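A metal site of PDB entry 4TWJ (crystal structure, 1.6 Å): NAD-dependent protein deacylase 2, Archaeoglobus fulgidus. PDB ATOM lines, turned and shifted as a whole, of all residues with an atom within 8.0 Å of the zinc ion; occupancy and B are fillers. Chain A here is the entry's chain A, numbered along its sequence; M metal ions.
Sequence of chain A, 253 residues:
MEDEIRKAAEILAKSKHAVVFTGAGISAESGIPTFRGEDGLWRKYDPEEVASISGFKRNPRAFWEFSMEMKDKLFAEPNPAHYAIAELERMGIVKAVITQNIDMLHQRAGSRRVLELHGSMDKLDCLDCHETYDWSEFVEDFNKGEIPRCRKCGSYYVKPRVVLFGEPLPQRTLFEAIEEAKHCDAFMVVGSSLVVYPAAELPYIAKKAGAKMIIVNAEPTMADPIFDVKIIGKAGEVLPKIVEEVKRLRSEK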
ATOM      1  N   ASP A 125      10.104  13.179 -22.476  1.00  0.00           N
ATOM      2  CA  ASP A 125       8.850  12.510 -22.826  1.00  0.00           C
ATOM      3  C   ASP A 125       8.535  11.403 -21.831  1.00  0.00           C
ATOM      4  O   ASP A 125       9.436  10.678 -21.417  1.00  0.00           O
ATOM      5  CB  ASP A 125       8.962  11.870 -24.204  1.00  0.00           C
ATOM      6  CG  ASP A 125       9.265  12.874 -25.289  1.00  0.00           C
ATOM      7  OD1 ASP A 125       8.327  13.515 -25.801  1.00  0.00           O
ATOM      8  OD2 ASP A 125      10.452  13.004 -25.643  1.00  0.00           O
ATOM      9  N   CYS A 126       7.271  11.272 -21.479  1.00  0.00           N
ATOM     10  CA  CYS A 126       6.812  10.096 -20.749  1.00  0.00           C
ATOM     11  C   CYS A 126       6.609   8.944 -21.726  1.00  0.00           C
ATOM     12  O   CYS A 126       5.839   9.070 -22.679  1.00  0.00           O
ATOM     13  CB  CYS A 126       5.512  10.386 -20.016  1.00  0.00           C
ATOM     14  SG  CYS A 126       4.785   8.930 -19.234  1.00  0.00           S
ATOM     15  N   LEU A 127       7.295   7.832 -21.501  1.00  0.00           N
ATOM     16  CA  LEU A 127       7.217   6.687 -22.410  1.00  0.00           C
ATOM     17  C   LEU A 127       5.874   5.968 -22.378  1.00  0.00           C
ATOM     18  O   LEU A 127       5.547   5.233 -23.310  1.00  0.00           O
ATOM     19  CB  LEU A 127       8.334   5.676 -22.112  1.00  0.00           C
ATOM     20  CG  LEU A 127       9.780   6.184 -22.162  1.00  0.00           C
ATOM     21  CD1 LEU A 127      10.746   5.009 -22.050  1.00  0.00           C
ATOM     22  CD2 LEU A 127      10.062   6.981 -23.430  1.00  0.00           C
ATOM     23  N   ASP A 128       5.106   6.164 -21.313  1.00  0.00           N
ATOM     24  CA  ASP A 128       3.802   5.495 -21.175  1.00  0.00           C
ATOM     25  C   ASP A 128       2.647   6.257 -21.821  1.00  0.00           C
ATOM     26  O   ASP A 128       1.907   5.671 -22.612  1.00  0.00           O
ATOM     27  CB  ASP A 128       3.504   5.223 -19.694  1.00  0.00           C
ATOM     28  CG  ASP A 128       4.294   4.053 -19.142  1.00  0.00           C
ATOM     29  OD1 ASP A 128       4.825   4.177 -18.016  1.00  0.00           O
ATOM     30  OD2 ASP A 128       4.396   3.008 -19.823  1.00  0.00           O
ATOM     31  N   CYS A 129       2.496   7.541 -21.501  1.00  0.00           N
ATOM     32  CA  CYS A 129       1.381   8.337 -22.047  1.00  0.00           C
ATOM     33  C   CYS A 129       1.815   9.404 -23.066  1.00  0.00           C
ATOM     34  O   CYS A 129       0.962  10.111 -23.612  1.00  0.00           O
ATOM     35  CB  CYS A 129       0.592   8.996 -20.912  1.00  0.00           C
ATOM     36  SG  CYS A 129       1.335  10.497 -20.255  1.00  0.00           S
ATOM     37  N   HIS A 130       3.120   9.505 -23.311  1.00  0.00           N
ATOM     38  CA  HIS A 130       3.692  10.373 -24.370  1.00  0.00           C
ATOM     39  C   HIS A 130       3.574  11.879 -24.084  1.00  0.00           C
ATOM     40  O   HIS A 130       3.753  12.707 -24.975  1.00  0.00           O
ATOM     41  CB  HIS A 130       3.092  10.004 -25.735  1.00  0.00           C
ATOM     42  CG  HIS A 130       2.980   8.533 -25.968  1.00  0.00           C
ATOM     43  ND1 HIS A 130       4.068   7.742 -26.267  1.00  0.00           N
ATOM     44  CD2 HIS A 130       1.903   7.699 -25.917  1.00  0.00           C
ATOM     45  CE1 HIS A 130       3.670   6.486 -26.397  1.00  0.00           C
ATOM     46  NE2 HIS A 130       2.374   6.434 -26.194  1.00  0.00           N
ATOM     47  N   GLU A 131       3.325  12.227 -22.828  1.00  0.00           N
ATOM     48  CA  GLU A 131       3.346  13.621 -22.389  1.00  0.00           C
ATOM     49  C   GLU A 131       4.744  14.211 -22.587  1.00  0.00           C
ATOM     50  O   GLU A 131       5.734  13.508 -22.398  1.00  0.00           O
ATOM     51  CB  GLU A 131       2.954  13.714 -20.915  1.00  0.00           C
ATOM     52  CG  GLU A 131       2.568  15.105 -20.438  1.00  0.00           C
ATOM     53  CD  GLU A 131       1.225  15.585 -20.971  1.00  0.00           C
ATOM     54  OE1 GLU A 131       0.541  14.859 -21.720  1.00  0.00           O
ATOM     55  OE2 GLU A 131       0.839  16.717 -20.629  1.00  0.00           O
ATOM     56  N   THR A 132       4.811  15.485 -22.969  1.00  0.00           N
ATOM     57  CA  THR A 132       6.092  16.157 -23.188  1.00  0.00           C
ATOM     58  C   THR A 132       6.371  17.191 -22.109  1.00  0.00           C
ATOM     59  O   THR A 132       5.452  17.786 -21.542  1.00  0.00           O
ATOM     60  CB  THR A 132       6.168  16.822 -24.572  1.00  0.00           C
ATOM     61  OG1 THR A 132       5.197  17.881 -24.644  1.00  0.00           O
ATOM     62  CG2 THR A 132       5.899  15.813 -25.665  1.00  0.00           C
ATOM     63  N   TYR A 133       7.664  17.389 -21.818  1.00  0.00           N
ATOM     64  CA  TYR A 133       8.104  18.284 -20.751  1.00  0.00           C
ATOM     65  C   TYR A 133       9.330  19.085 -21.144  1.00  0.00           C
ATOM     66  O   TYR A 133      10.114  18.651 -21.989  1.00  0.00           O
ATOM     67  CB  TYR A 133       8.473  17.474 -19.493  1.00  0.00           C
ATOM     68  CG  TYR A 133       7.320  16.729 -18.888  1.00  0.00           C
ATOM     69  CD1 TYR A 133       7.016  15.441 -19.295  1.00  0.00           C
ATOM     70  CD2 TYR A 133       6.529  17.328 -17.920  1.00  0.00           C
ATOM     71  CE1 TYR A 133       5.950  14.752 -18.744  1.00  0.00           C
ATOM     72  CE2 TYR A 133       5.456  16.661 -17.367  1.00  0.00           C
ATOM     73  CZ  TYR A 133       5.163  15.377 -17.781  1.00  0.00           C
ATOM     74  OH  TYR A 133       4.088  14.727 -17.222  1.00  0.00           O
ATOM     75  N   ARG A 149       8.889  12.394 -12.527  1.00  0.00           N
ATOM     76  CA  ARG A 149       7.733  11.516 -12.661  1.00  0.00           C
ATOM     77  C   ARG A 149       6.761  12.233 -13.573  1.00  0.00           C
ATOM     78  O   ARG A 149       6.693  13.458 -13.562  1.00  0.00           O
ATOM     79  CB  ARG A 149       7.071  11.299 -11.297  1.00  0.00           C
ATOM     80  CG  ARG A 149       7.898  10.524 -10.290  1.00  0.00           C
ATOM     81  CD  ARG A 149       7.864   9.020 -10.511  1.00  0.00           C
ATOM     82  NE  ARG A 149       6.513   8.458 -10.390  1.00  0.00           N
ATOM     83  CZ  ARG A 149       5.917   8.115  -9.245  1.00  0.00           C
ATOM     84  NH1 ARG A 149       6.509   8.260  -8.063  1.00  0.00           N
ATOM     85  NH2 ARG A 149       4.678   7.606  -9.279  1.00  0.00           N
ATOM     86  N   CYS A 150       6.009  11.473 -14.368  1.00  0.00           N
ATOM     87  CA  CYS A 150       5.010  12.079 -15.229  1.00  0.00           C
ATOM     88  C   CYS A 150       3.835  12.587 -14.394  1.00  0.00           C
ATOM     89  O   CYS A 150       3.229  11.818 -13.651  1.00  0.00           O
ATOM     90  CB  CYS A 150       4.504  11.075 -16.240  1.00  0.00           C
ATOM     91  SG  CYS A 150       3.286  11.754 -17.383  1.00  0.00           S
ATOM     92  N   ARG A 151       3.530  13.875 -14.500  1.00  0.00           N
ATOM     93  CA  ARG A 151       2.439  14.458 -13.726  1.00  0.00           C
ATOM     94  C   ARG A 151       1.079  13.970 -14.220  1.00  0.00           C
ATOM     95  O   ARG A 151       0.153  13.815 -13.418  1.00  0.00           O
ATOM     96  CB  ARG A 151       2.507  15.980 -13.766  1.00  0.00           C
ATOM     97  CG  ARG A 151       1.435  16.657 -12.905  1.00  0.00           C
ATOM     98  CD  ARG A 151       1.666  18.157 -12.829  1.00  0.00           C
ATOM     99  NE  ARG A 151       2.817  18.512 -11.998  1.00  0.00           N
ATOM    100  CZ  ARG A 151       2.759  18.980 -10.742  1.00  0.00           C
ATOM    101  NH1 ARG A 151       3.894  19.285 -10.110  1.00  0.00           N
ATOM    102  NH2 ARG A 151       1.600  19.167 -10.120  1.00  0.00           N
ATOM    103  N   LYS A 152       0.944  13.725 -15.513  1.00  0.00           N
ATOM    104  CA  LYS A 152      -0.336  13.286 -16.063  1.00  0.00           C
ATOM    105  C   LYS A 152      -0.706  11.897 -15.564  1.00  0.00           C
ATOM    106  O   LYS A 152      -1.780  11.711 -14.982  1.00  0.00           O
ATOM    107  CB  LYS A 152      -0.327  13.314 -17.591  1.00  0.00           C
ATOM    108  CG  LYS A 152      -1.640  12.853 -18.207  1.00  0.00           C
ATOM    109  CD  LYS A 152      -1.724  13.153 -19.693  1.00  0.00           C
ATOM    110  CE  LYS A 152      -2.088  14.614 -19.941  1.00  0.00           C
ATOM    111  NZ  LYS A 152      -2.174  14.907 -21.392  1.00  0.00           N
ATOM    112  N   CYS A 153       0.172  10.917 -15.773  1.00  0.00           N
ATOM    113  CA  CYS A 153      -0.162   9.511 -15.525  1.00  0.00           C
ATOM    114  C   CYS A 153       0.580   8.864 -14.342  1.00  0.00           C
ATOM    115  O   CYS A 153       0.232   7.745 -13.940  1.00  0.00           O
ATOM    116  CB  CYS A 153       0.070   8.697 -16.788  1.00  0.00           C
ATOM    117  SG  CYS A 153       1.787   8.233 -17.096  1.00  0.00           S
ATOM    118  N   GLY A 154       1.574   9.564 -13.793  1.00  0.00           N
ATOM    119  CA  GLY A 154       2.308   9.086 -12.613  1.00  0.00           C
ATOM    120  C   GLY A 154       3.506   8.195 -12.912  1.00  0.00           C
ATOM    121  O   GLY A 154       4.182   7.750 -11.996  1.00  0.00           O
ATOM    122  N   SER A 155       3.778   7.954 -14.198  1.00  0.00           N
ATOM    123  CA  SER A 155       4.826   7.018 -14.601  1.00  0.00           C
ATOM    124  C   SER A 155       6.209   7.391 -14.076  1.00  0.00           C
ATOM    125  O   SER A 155       6.536   8.564 -13.911  1.00  0.00           O
ATOM    126  CB  SER A 155       4.883   6.893 -16.122  1.00  0.00           C
ATOM    127  OG  SER A 155       5.909   6.003 -16.536  1.00  0.00           O
ATOM    128  N   TYR A 156       7.014   6.356 -13.839  1.00  0.00           N
ATOM    129  CA  TYR A 156       8.428   6.516 -13.525  1.00  0.00           C
ATOM    130  C   TYR A 156       9.289   6.644 -14.794  1.00  0.00           C
ATOM    131  O   TYR A 156      10.505   6.817 -14.703  1.00  0.00           O
ATOM    132  CB  TYR A 156       8.939   5.304 -12.718  1.00  0.00           C
ATOM    133  CG  TYR A 156       8.635   5.354 -11.236  1.00  0.00           C
ATOM    134  CD1 TYR A 156       9.641   5.650 -10.310  1.00  0.00           C
ATOM    135  CD2 TYR A 156       7.355   5.076 -10.749  1.00  0.00           C
ATOM    136  CE1 TYR A 156       9.370   5.694  -8.947  1.00  0.00           C
ATOM    137  CE2 TYR A 156       7.087   5.104  -9.392  1.00  0.00           C
ATOM    138  CZ  TYR A 156       8.102   5.413  -8.499  1.00  0.00           C
ATOM    139  OH  TYR A 156       7.834   5.441  -7.143  1.00  0.00           O
ATOM    140  N   TYR A 157       8.661   6.556 -15.975  1.00  0.00           N
ATOM    141  CA  TYR A 157       9.404   6.508 -17.240  1.00  0.00           C
ATOM    142  C   TYR A 157       9.403   7.840 -17.989  1.00  0.00           C
ATOM    143  O   TYR A 157       8.945   7.919 -19.135  1.00  0.00           O
ATOM    144  CB  TYR A 157       8.868   5.379 -18.129  1.00  0.00           C
ATOM    145  CG  TYR A 157       9.195   4.012 -17.616  1.00  0.00           C
ATOM    146  CD1 TYR A 157       8.388   3.390 -16.665  1.00  0.00           C
ATOM    147  CD2 TYR A 157      10.321   3.340 -18.054  1.00  0.00           C
ATOM    148  CE1 TYR A 157       8.698   2.131 -16.178  1.00  0.00           C
ATOM    149  CE2 TYR A 157      10.635   2.078 -17.576  1.00  0.00           C
ATOM    150  CZ  TYR A 157       9.829   1.475 -16.641  1.00  0.00           C
ATOM    151  OH  TYR A 157      10.149   0.224 -16.174  1.00  0.00           O
ATOM    152  N   VAL A 158       9.931   8.873 -17.339  1.00  0.00           N
ATOM    153  CA  VAL A 158      10.177  10.157 -18.005  1.00  0.00           C
ATOM    154  C   VAL A 158      11.580  10.107 -18.572  1.00  0.00           C
ATOM    155  O   VAL A 158      12.566  10.116 -17.828  1.00  0.00           O
ATOM    156  CB  VAL A 158      10.041  11.350 -17.038  1.00  0.00           C
ATOM    157  CG1 VAL A 158      10.365  12.653 -17.763  1.00  0.00           C
ATOM    158  CG2 VAL A 158       8.645  11.383 -16.440  1.00  0.00           C
HETATM  159 ZN    ZN M   1       2.746   9.808 -18.541  1.00  0.00          ZN
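Four residues have an atom within 4 Å of the zinc ion: Cys 126, Cys 129, Cys 150 and Cys 153.
The nearest printed residue that does not touch the zinc ion is Ser 155 (4.3 Å).
The zinc ion is bound by the side-chain sulfur of Cys 129 (2.3 Å), the side-chain sulfur of Cys 126 (2.3 Å), the side-chain sulfur of Cys 150 (2.3 Å) and the side-chain sulfur of Cys 153 (2.3 Å).
The zinc ion has four donor atoms within binding distance.
The side-chain sulfur (SG) of Cys 129 sits close to the backbone NH (N) of Glu 131, at 3.7 Å.
O of Glu 131 is in hydrogen-bond range of N of Cys 126 (2.9 Å).
SG of Cys 126 sits close to N of Asp 128, at 3.5 Å.
The backbone NH (N) of Cys 150 lies within hydrogen-bond range of the backbone carbonyl oxygen (O) of Ser 155 (3.0 Å).
The side-chain sulfur (SG) of Cys 150 sits close to the backbone NH (N) of Lys 152 (3.6 Å).
The side-chain sulfur (SG) of Cys 150 sits close to the side-chain hydroxyl (OH) of Tyr 133, at 3.1 Å.
SG of Cys 153 lies close to N of Ser 155, at 3.5 Å.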
